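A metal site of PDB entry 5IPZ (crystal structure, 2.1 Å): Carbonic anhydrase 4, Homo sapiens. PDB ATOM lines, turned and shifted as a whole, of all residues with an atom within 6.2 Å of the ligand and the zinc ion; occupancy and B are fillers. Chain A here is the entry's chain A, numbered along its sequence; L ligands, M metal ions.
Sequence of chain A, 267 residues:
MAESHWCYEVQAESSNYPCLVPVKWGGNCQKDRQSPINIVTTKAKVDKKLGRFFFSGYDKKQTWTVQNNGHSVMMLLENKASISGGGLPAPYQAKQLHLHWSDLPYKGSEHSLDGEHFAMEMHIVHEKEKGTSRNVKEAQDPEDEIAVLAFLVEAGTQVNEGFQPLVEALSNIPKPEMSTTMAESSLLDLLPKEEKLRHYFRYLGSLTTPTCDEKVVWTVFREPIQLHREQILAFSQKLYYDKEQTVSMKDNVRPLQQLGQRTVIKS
A nitrogen (N1) of the ligand lies close to the side-chain hydroxyl (OG1) of Thr 208, at 2.8 Å.
O2 of the ligand is in hydrogen-bond range of N of Thr 208 (3.0 Å).
ND2 of Asn 69 sits close to S2 of the ligand (3.3 Å).
Merely in contact with the zinc ion: Thr 208 (3.98 Å).
Within 4 Å of the zinc ion: His 98, His 100, His 123 and Thr 208.
Merely in contact with the ligand: Leu 207 (2.8 Å), Gln 96 (3.2 Å), Val 148 (3.4 Å), Thr 209 (3.5 Å), Val 125 (3.5 Å), Trp 218 (3.6 Å) and Met 74 (3.7 Å).
Hydrophobic or aromatic side chains within 4 Å of the ligand: Met 74, His 98, His 100, His 123, Val 125, Val 148, Leu 207 and Trp 218.
12 residues have an atom within 4 Å of the ligand: Asn 69, Met 74, Gln 96, His 98, His 100, His 123, Val 125, Val 148, Leu 207, Thr 208, Thr 209 and Trp 218.
A ring nitrogen (ND1) of His 98 lies within hydrogen-bond range of the side-chain amide oxygen (OE1) of Gln 96 (2.9 Å).
OD1 of Asn 69 lies within hydrogen-bond range of N of His 71.
N of Glu 121 is in hydrogen-bond range of O of His 100 (2.7 Å).
NE2 of His 123 lies within hydrogen-bond range of OE2 of Glu 121 (2.6 Å).
OD1 of Asn 69 lies within hydrogen-bond range of N of Ser 72.
The backbone NH (N) of Val 125 lies within hydrogen-bond range of the backbone carbonyl oxygen (O) of Gln 96, 2.9 Å away.
The side-chain hydroxyl of Thr 208 is in hydrogen-bond range of the side-chain carboxylate of Glu 110 (2.6 Å).
NE2 of His 100 lies close to OE1 of Glu 110, 3.3 Å away.
The zinc ion is bound by NE2 of His 98 (1.9 Å), ND1 of His 123 (1.9 Å), N1 of the ligand (1.9 Å) and NE2 of His 100 (2.0 Å).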
ATOM      1  N   TRP A   6      28.549 -26.662 -28.683  1.00  0.00           N
ATOM      2  CA  TRP A   6      27.248 -27.256 -28.972  1.00  0.00           C
ATOM      3  C   TRP A   6      26.223 -26.146 -29.010  1.00  0.00           C
ATOM      4  O   TRP A   6      26.454 -25.066 -28.486  1.00  0.00           O
ATOM      5  CB  TRP A   6      26.863 -28.289 -27.964  1.00  0.00           C
ATOM      6  CG  TRP A   6      26.800 -27.772 -26.530  1.00  0.00           C
ATOM      7  CD1 TRP A   6      27.824 -27.749 -25.579  1.00  0.00           C
ATOM      8  CD2 TRP A   6      25.631 -27.178 -25.845  1.00  0.00           C
ATOM      9  NE1 TRP A   6      27.386 -27.199 -24.397  1.00  0.00           N
ATOM     10  CE2 TRP A   6      26.071 -26.835 -24.490  1.00  0.00           C
ATOM     11  CE3 TRP A   6      24.306 -26.911 -26.207  1.00  0.00           C
ATOM     12  CZ2 TRP A   6      25.216 -26.261 -23.563  1.00  0.00           C
ATOM     13  CZ3 TRP A   6      23.467 -26.323 -25.267  1.00  0.00           C
ATOM     14  CH2 TRP A   6      23.901 -26.012 -23.972  1.00  0.00           C
ATOM     15  N   TYR A   8      21.626 -25.140 -29.607  1.00  0.00           N
ATOM     16  CA  TYR A   8      20.208 -25.572 -29.593  1.00  0.00           C
ATOM     17  C   TYR A   8      19.739 -25.505 -31.030  1.00  0.00           C
ATOM     18  O   TYR A   8      20.350 -24.802 -31.841  1.00  0.00           O
ATOM     19  CB  TYR A   8      19.333 -24.661 -28.680  1.00  0.00           C
ATOM     20  CG  TYR A   8      19.479 -24.996 -27.199  1.00  0.00           C
ATOM     21  CD1 TYR A   8      19.028 -26.222 -26.703  1.00  0.00           C
ATOM     22  CD2 TYR A   8      20.127 -24.134 -26.307  1.00  0.00           C
ATOM     23  CE1 TYR A   8      19.180 -26.568 -25.365  1.00  0.00           C
ATOM     24  CE2 TYR A   8      20.293 -24.475 -24.954  1.00  0.00           C
ATOM     25  CZ  TYR A   8      19.818 -25.704 -24.502  1.00  0.00           C
ATOM     26  OH  TYR A   8      19.955 -26.073 -23.175  1.00  0.00           O
ATOM     27  N   ASN A  69      25.842 -17.420 -19.842  1.00  0.00           N
ATOM     28  CA  ASN A  69      26.893 -18.337 -20.265  1.00  0.00           C
ATOM     29  C   ASN A  69      26.737 -18.665 -21.756  1.00  0.00           C
ATOM     30  O   ASN A  69      27.327 -19.632 -22.237  1.00  0.00           O
ATOM     31  CB  ASN A  69      26.815 -19.614 -19.454  1.00  0.00           C
ATOM     32  CG  ASN A  69      25.493 -20.330 -19.644  1.00  0.00           C
ATOM     33  OD1 ASN A  69      24.692 -19.884 -20.461  1.00  0.00           O
ATOM     34  ND2 ASN A  69      25.262 -21.463 -18.935  1.00  0.00           N
ATOM     35  N   HIS A  71      24.166 -20.040 -23.048  1.00  0.00           N
ATOM     36  CA  HIS A  71      23.132 -21.070 -23.219  1.00  0.00           C
ATOM     37  C   HIS A  71      21.891 -20.846 -22.395  1.00  0.00           C
ATOM     38  O   HIS A  71      20.776 -21.282 -22.768  1.00  0.00           O
ATOM     39  CB  HIS A  71      23.669 -22.435 -22.900  1.00  0.00           C
ATOM     40  CG  HIS A  71      24.844 -22.841 -23.740  1.00  0.00           C
ATOM     41  ND1 HIS A  71      24.768 -22.938 -25.076  1.00  0.00           N
ATOM     42  CD2 HIS A  71      26.133 -23.202 -23.379  1.00  0.00           C
ATOM     43  CE1 HIS A  71      25.966 -23.351 -25.552  1.00  0.00           C
ATOM     44  NE2 HIS A  71      26.792 -23.524 -24.506  1.00  0.00           N
ATOM     45  N   SER A  72      22.098 -20.206 -21.239  1.00  0.00           N
ATOM     46  CA  SER A  72      21.038 -19.896 -20.346  1.00  0.00           C
ATOM     47  C   SER A  72      21.478 -18.656 -19.546  1.00  0.00           C
ATOM     48  O   SER A  72      22.559 -18.122 -19.787  1.00  0.00           O
ATOM     49  CB  SER A  72      20.868 -21.050 -19.390  1.00  0.00           C
ATOM     50  OG  SER A  72      19.708 -20.795 -18.637  1.00  0.00           O
ATOM     51  N   MET A  74      22.429 -18.086 -15.557  1.00  0.00           N
ATOM     52  CA  MET A  74      22.718 -18.965 -14.424  1.00  0.00           C
ATOM     53  C   MET A  74      23.118 -18.170 -13.186  1.00  0.00           C
ATOM     54  O   MET A  74      23.986 -17.284 -13.266  1.00  0.00           O
ATOM     55  CB  MET A  74      23.892 -19.846 -14.783  1.00  0.00           C
ATOM     56  CG  MET A  74      24.172 -20.986 -13.842  1.00  0.00           C
ATOM     57  SD  MET A  74      25.631 -21.901 -14.409  1.00  0.00           S
ATOM     58  CE  MET A  74      24.876 -23.418 -14.924  1.00  0.00           C
ATOM     59  N   GLN A  96      23.811 -24.308  -8.599  1.00  0.00           N
ATOM     60  CA  GLN A  96      23.437 -23.265  -9.532  1.00  0.00           C
ATOM     61  C   GLN A  96      21.913 -23.369  -9.871  1.00  0.00           C
ATOM     62  O   GLN A  96      21.277 -24.346  -9.522  1.00  0.00           O
ATOM     63  CB  GLN A  96      24.359 -23.306 -10.770  1.00  0.00           C
ATOM     64  CG  GLN A  96      24.524 -24.693 -11.379  1.00  0.00           C
ATOM     65  CD  GLN A  96      23.641 -24.873 -12.613  1.00  0.00           C
ATOM     66  OE1 GLN A  96      22.667 -24.134 -12.808  1.00  0.00           O
ATOM     67  NE2 GLN A  96      23.972 -25.867 -13.456  1.00  0.00           N
ATOM     68  N   HIS A  98      19.272 -22.130 -13.111  1.00  0.00           N
ATOM     69  CA  HIS A  98      19.175 -21.572 -14.438  1.00  0.00           C
ATOM     70  C   HIS A  98      17.814 -21.866 -15.001  1.00  0.00           C
ATOM     71  O   HIS A  98      17.043 -22.602 -14.400  1.00  0.00           O
ATOM     72  CB  HIS A  98      20.264 -22.207 -15.341  1.00  0.00           C
ATOM     73  CG  HIS A  98      20.083 -23.696 -15.598  1.00  0.00           C
ATOM     74  ND1 HIS A  98      20.729 -24.619 -14.894  1.00  0.00           N
ATOM     75  CD2 HIS A  98      19.314 -24.387 -16.542  1.00  0.00           C
ATOM     76  CE1 HIS A  98      20.390 -25.855 -15.312  1.00  0.00           C
ATOM     77  NE2 HIS A  98      19.563 -25.731 -16.373  1.00  0.00           N
ATOM     78  N   LEU A  99      17.507 -21.314 -16.187  1.00  0.00           N
ATOM     79  CA  LEU A  99      16.174 -21.409 -16.723  1.00  0.00           C
ATOM     80  C   LEU A  99      16.230 -21.838 -18.183  1.00  0.00           C
ATOM     81  O   LEU A  99      17.271 -21.735 -18.795  1.00  0.00           O
ATOM     82  CB  LEU A  99      15.426 -20.094 -16.579  1.00  0.00           C
ATOM     83  CG  LEU A  99      15.219 -19.585 -15.137  1.00  0.00           C
ATOM     84  CD1 LEU A  99      16.304 -18.550 -14.854  1.00  0.00           C
ATOM     85  CD2 LEU A  99      13.837 -19.008 -14.926  1.00  0.00           C
ATOM     86  N   HIS A 100      15.100 -22.321 -18.719  1.00  0.00           N
ATOM     87  CA  HIS A 100      14.954 -22.492 -20.185  1.00  0.00           C
ATOM     88  C   HIS A 100      13.703 -21.812 -20.539  1.00  0.00           C
ATOM     89  O   HIS A 100      12.770 -21.851 -19.729  1.00  0.00           O
ATOM     90  CB  HIS A 100      14.873 -23.996 -20.520  1.00  0.00           C
ATOM     91  CG  HIS A 100      16.046 -24.787 -19.959  1.00  0.00           C
ATOM     92  ND1 HIS A 100      17.149 -25.047 -20.678  1.00  0.00           N
ATOM     93  CD2 HIS A 100      16.239 -25.377 -18.728  1.00  0.00           C
ATOM     94  CE1 HIS A 100      18.003 -25.750 -19.969  1.00  0.00           C
ATOM     95  NE2 HIS A 100      17.458 -25.959 -18.754  1.00  0.00           N
ATOM     96  N   GLU A 110      11.105 -27.679 -20.813  1.00  0.00           N
ATOM     97  CA  GLU A 110      11.804 -28.884 -21.278  1.00  0.00           C
ATOM     98  C   GLU A 110      11.013 -30.096 -20.905  1.00  0.00           C
ATOM     99  O   GLU A 110      10.833 -31.035 -21.732  1.00  0.00           O
ATOM    100  CB  GLU A 110      13.201 -29.013 -20.670  1.00  0.00           C
ATOM    101  CG  GLU A 110      14.147 -27.902 -21.085  1.00  0.00           C
ATOM    102  CD  GLU A 110      15.631 -28.350 -21.069  1.00  0.00           C
ATOM    103  OE1 GLU A 110      16.151 -28.768 -20.028  1.00  0.00           O
ATOM    104  OE2 GLU A 110      16.263 -28.252 -22.131  1.00  0.00           O
ATOM    105  N   GLU A 121      11.132 -23.083 -18.002  1.00  0.00           N
ATOM    106  CA  GLU A 121      11.367 -23.995 -16.915  1.00  0.00           C
ATOM    107  C   GLU A 121      12.667 -23.719 -16.151  1.00  0.00           C
ATOM    108  O   GLU A 121      13.724 -23.654 -16.717  1.00  0.00           O
ATOM    109  CB  GLU A 121      11.250 -25.417 -17.415  1.00  0.00           C
ATOM    110  CG  GLU A 121      11.633 -26.492 -16.419  1.00  0.00           C
ATOM    111  CD  GLU A 121      11.614 -27.874 -17.055  1.00  0.00           C
ATOM    112  OE1 GLU A 121      10.916 -28.038 -18.060  1.00  0.00           O
ATOM    113  OE2 GLU A 121      12.304 -28.813 -16.558  1.00  0.00           O
ATOM    114  N   HIS A 123      15.486 -24.661 -13.287  1.00  0.00           N
ATOM    115  CA  HIS A 123      16.289 -25.723 -12.726  1.00  0.00           C
ATOM    116  C   HIS A 123      17.202 -25.309 -11.606  1.00  0.00           C
ATOM    117  O   HIS A 123      18.115 -24.482 -11.783  1.00  0.00           O
ATOM    118  CB  HIS A 123      17.161 -26.375 -13.836  1.00  0.00           C
ATOM    119  CG  HIS A 123      16.361 -27.049 -14.917  1.00  0.00           C
ATOM    120  ND1 HIS A 123      16.848 -27.347 -16.131  1.00  0.00           N
ATOM    121  CD2 HIS A 123      15.051 -27.538 -14.890  1.00  0.00           C
ATOM    122  CE1 HIS A 123      15.878 -27.959 -16.870  1.00  0.00           C
ATOM    123  NE2 HIS A 123      14.793 -28.076 -16.097  1.00  0.00           N
ATOM    124  N   ILE A 124      17.015 -25.899 -10.453  1.00  0.00           N
ATOM    125  CA  ILE A 124      17.951 -25.676  -9.352  1.00  0.00           C
ATOM    126  C   ILE A 124      18.682 -26.970  -9.150  1.00  0.00           C
ATOM    127  O   ILE A 124      18.051 -27.952  -8.785  1.00  0.00           O
ATOM    128  CB  ILE A 124      17.240 -25.211  -8.049  1.00  0.00           C
ATOM    129  CG1 ILE A 124      16.113 -24.206  -8.395  1.00  0.00           C
ATOM    130  CG2 ILE A 124      18.284 -24.632  -7.065  1.00  0.00           C
ATOM    131  CD1 ILE A 124      15.260 -23.726  -7.196  1.00  0.00           C
ATOM    132  N   VAL A 125      19.999 -26.933  -9.449  1.00  0.00           N
ATOM    133  CA  VAL A 125      20.928 -28.079  -9.590  1.00  0.00           C
ATOM    134  C   VAL A 125      21.662 -28.224  -8.224  1.00  0.00           C
ATOM    135  O   VAL A 125      22.279 -27.264  -7.746  1.00  0.00           O
ATOM    136  CB  VAL A 125      21.941 -27.822 -10.812  1.00  0.00           C
ATOM    137  CG1 VAL A 125      23.008 -28.897 -10.932  1.00  0.00           C
ATOM    138  CG2 VAL A 125      21.208 -27.728 -12.170  1.00  0.00           C
ATOM    139  N   ILE A 146      23.540 -36.008  -8.875  1.00  0.00           N
ATOM    140  CA  ILE A 146      22.973 -34.672  -8.985  1.00  0.00           C
ATOM    141  C   ILE A 146      21.479 -34.691  -8.761  1.00  0.00           C
ATOM    142  O   ILE A 146      20.825 -35.627  -9.183  1.00  0.00           O
ATOM    143  CB  ILE A 146      23.350 -33.993 -10.323  1.00  0.00           C
ATOM    144  CG1 ILE A 146      24.746 -33.368 -10.191  1.00  0.00           C
ATOM    145  CG2 ILE A 146      22.349 -32.913 -10.701  1.00  0.00           C
ATOM    146  CD1 ILE A 146      25.212 -32.671 -11.461  1.00  0.00           C
ATOM    147  N   VAL A 148      18.164 -32.394  -9.414  1.00  0.00           N
ATOM    148  CA  VAL A 148      17.582 -31.181  -9.983  1.00  0.00           C
ATOM    149  C   VAL A 148      16.144 -30.948  -9.497  1.00  0.00           C
ATOM    150  O   VAL A 148      15.316 -31.827  -9.564  1.00  0.00           O
ATOM    151  CB  VAL A 148      17.638 -31.120 -11.533  1.00  0.00           C
ATOM    152  CG1 VAL A 148      17.013 -29.821 -11.992  1.00  0.00           C
ATOM    153  CG2 VAL A 148      19.096 -31.124 -12.032  1.00  0.00           C
ATOM    154  N   SER A 206      19.137 -37.624 -16.946  1.00  0.00           N
ATOM    155  CA  SER A 206      20.420 -37.023 -17.344  1.00  0.00           C
ATOM    156  C   SER A 206      20.359 -35.508 -17.241  1.00  0.00           C
ATOM    157  O   SER A 206      19.285 -34.969 -16.980  1.00  0.00           O
ATOM    158  CB  SER A 206      20.835 -37.419 -18.784  1.00  0.00           C
ATOM    159  OG  SER A 206      20.102 -36.696 -19.763  1.00  0.00           O
ATOM    160  N   LEU A 207      21.483 -34.885 -17.522  1.00  0.00           N
ATOM    161  CA  LEU A 207      21.601 -33.428 -17.629  1.00  0.00           C
ATOM    162  C   LEU A 207      20.982 -33.219 -18.969  1.00  0.00           C
ATOM    163  O   LEU A 207      20.989 -34.145 -19.752  1.00  0.00           O
ATOM    164  CB  LEU A 207      23.060 -33.005 -17.715  1.00  0.00           C
ATOM    165  CG  LEU A 207      24.040 -33.076 -16.536  1.00  0.00           C
ATOM    166  CD1 LEU A 207      25.203 -32.126 -16.789  1.00  0.00           C
ATOM    167  CD2 LEU A 207      23.348 -32.749 -15.227  1.00  0.00           C
ATOM    168  N   THR A 208      20.431 -32.030 -19.247  1.00  0.00           N
ATOM    169  CA  THR A 208      19.701 -31.902 -20.512  1.00  0.00           C
ATOM    170  C   THR A 208      20.563 -31.132 -21.469  1.00  0.00           C
ATOM    171  O   THR A 208      20.100 -30.691 -22.494  1.00  0.00           O
ATOM    172  CB  THR A 208      18.341 -31.186 -20.380  1.00  0.00           C
ATOM    173  OG1 THR A 208      18.531 -29.844 -19.909  1.00  0.00           O
ATOM    174  CG2 THR A 208      17.397 -31.943 -19.464  1.00  0.00           C
ATOM    175  N   THR A 209      21.824 -30.929 -21.090  1.00  0.00           N
ATOM    176  CA  THR A 209      22.818 -30.293 -21.947  1.00  0.00           C
ATOM    177  C   THR A 209      24.077 -31.146 -21.918  1.00  0.00           C
ATOM    178  O   THR A 209      24.237 -31.969 -20.981  1.00  0.00           O
ATOM    179  CB  THR A 209      23.198 -28.891 -21.449  1.00  0.00           C
ATOM    180  OG1 THR A 209      23.862 -29.052 -20.201  1.00  0.00           O
ATOM    181  CG2 THR A 209      21.939 -28.017 -21.301  1.00  0.00           C
ATOM    182  N   VAL A 216      21.306 -37.974 -12.919  1.00  0.00           N
ATOM    183  CA  VAL A 216      20.355 -37.026 -12.300  1.00  0.00           C
ATOM    184  C   VAL A 216      19.129 -37.710 -11.737  1.00  0.00           C
ATOM    185  O   VAL A 216      18.420 -38.440 -12.453  1.00  0.00           O
ATOM    186  CB  VAL A 216      19.911 -35.941 -13.281  1.00  0.00           C
ATOM    187  CG1 VAL A 216      19.062 -34.898 -12.585  1.00  0.00           C
ATOM    188  CG2 VAL A 216      21.117 -35.255 -13.900  1.00  0.00           C
ATOM    189  N   TRP A 218      15.614 -36.781 -10.827  1.00  0.00           N
ATOM    190  CA  TRP A 218      14.783 -35.649 -11.231  1.00  0.00           C
ATOM    191  C   TRP A 218      13.600 -35.406 -10.342  1.00  0.00           C
ATOM    192  O   TRP A 218      13.021 -36.366  -9.846  1.00  0.00           O
ATOM    193  CB  TRP A 218      14.303 -35.808 -12.677  1.00  0.00           C
ATOM    194  CG  TRP A 218      15.337 -35.364 -13.673  1.00  0.00           C
ATOM    195  CD1 TRP A 218      16.273 -36.148 -14.340  1.00  0.00           C
ATOM    196  CD2 TRP A 218      15.600 -33.997 -14.111  1.00  0.00           C
ATOM    197  NE1 TRP A 218      17.061 -35.380 -15.144  1.00  0.00           N
ATOM    198  CE2 TRP A 218      16.710 -34.075 -15.063  1.00  0.00           C
ATOM    199  CE3 TRP A 218      15.040 -32.753 -13.831  1.00  0.00           C
ATOM    200  CZ2 TRP A 218      17.218 -32.951 -15.679  1.00  0.00           C
ATOM    201  CZ3 TRP A 218      15.566 -31.626 -14.464  1.00  0.00           C
ATOM    202  CH2 TRP A 218      16.635 -31.736 -15.364  1.00  0.00           C
HETATM  203  C1  LIG L   1      23.597 -25.780 -18.918  1.00  0.00           C
HETATM  204 CL1  LIG L   1      21.853 -30.674 -14.030  1.00  0.00          CL
HETATM  205  C2  LIG L   1      22.562 -29.421 -15.098  1.00  0.00           C
HETATM  206  C3  LIG L   1      21.849 -28.833 -16.153  1.00  0.00           C
HETATM  207  S1  LIG L   1      20.160 -29.313 -16.416  1.00  0.00           S
HETATM  208  O1  LIG L   1      19.392 -29.052 -15.069  1.00  0.00           O
HETATM  209  O2  LIG L   1      20.062 -30.839 -16.552  1.00  0.00           O
HETATM  210  N1  LIG L   1      19.385 -28.477 -17.680  1.00  0.00           N
HETATM  211  C4  LIG L   1      22.383 -27.852 -17.039  1.00  0.00           C
HETATM  212  C5  LIG L   1      23.909 -28.985 -14.971  1.00  0.00           C
HETATM  213  C6  LIG L   1      24.453 -28.004 -15.853  1.00  0.00           C
HETATM  214  C7  LIG L   1      23.704 -27.421 -16.899  1.00  0.00           C
HETATM  215  C8  LIG L   1      24.270 -26.370 -17.821  1.00  0.00           C
HETATM  216  N2  LIG L   1      25.541 -25.863 -17.628  1.00  0.00           N
HETATM  217  C9  LIG L   1      25.880 -24.936 -18.557  1.00  0.00           C
HETATM  218  N3  LIG L   1      27.138 -24.299 -18.538  1.00  0.00           N
HETATM  219  S2  LIG L   1      24.636 -24.669 -19.606  1.00  0.00           S
HETATM  220 ZN    ZN M   1      18.367 -26.910 -17.221  1.00  0.00          ZN
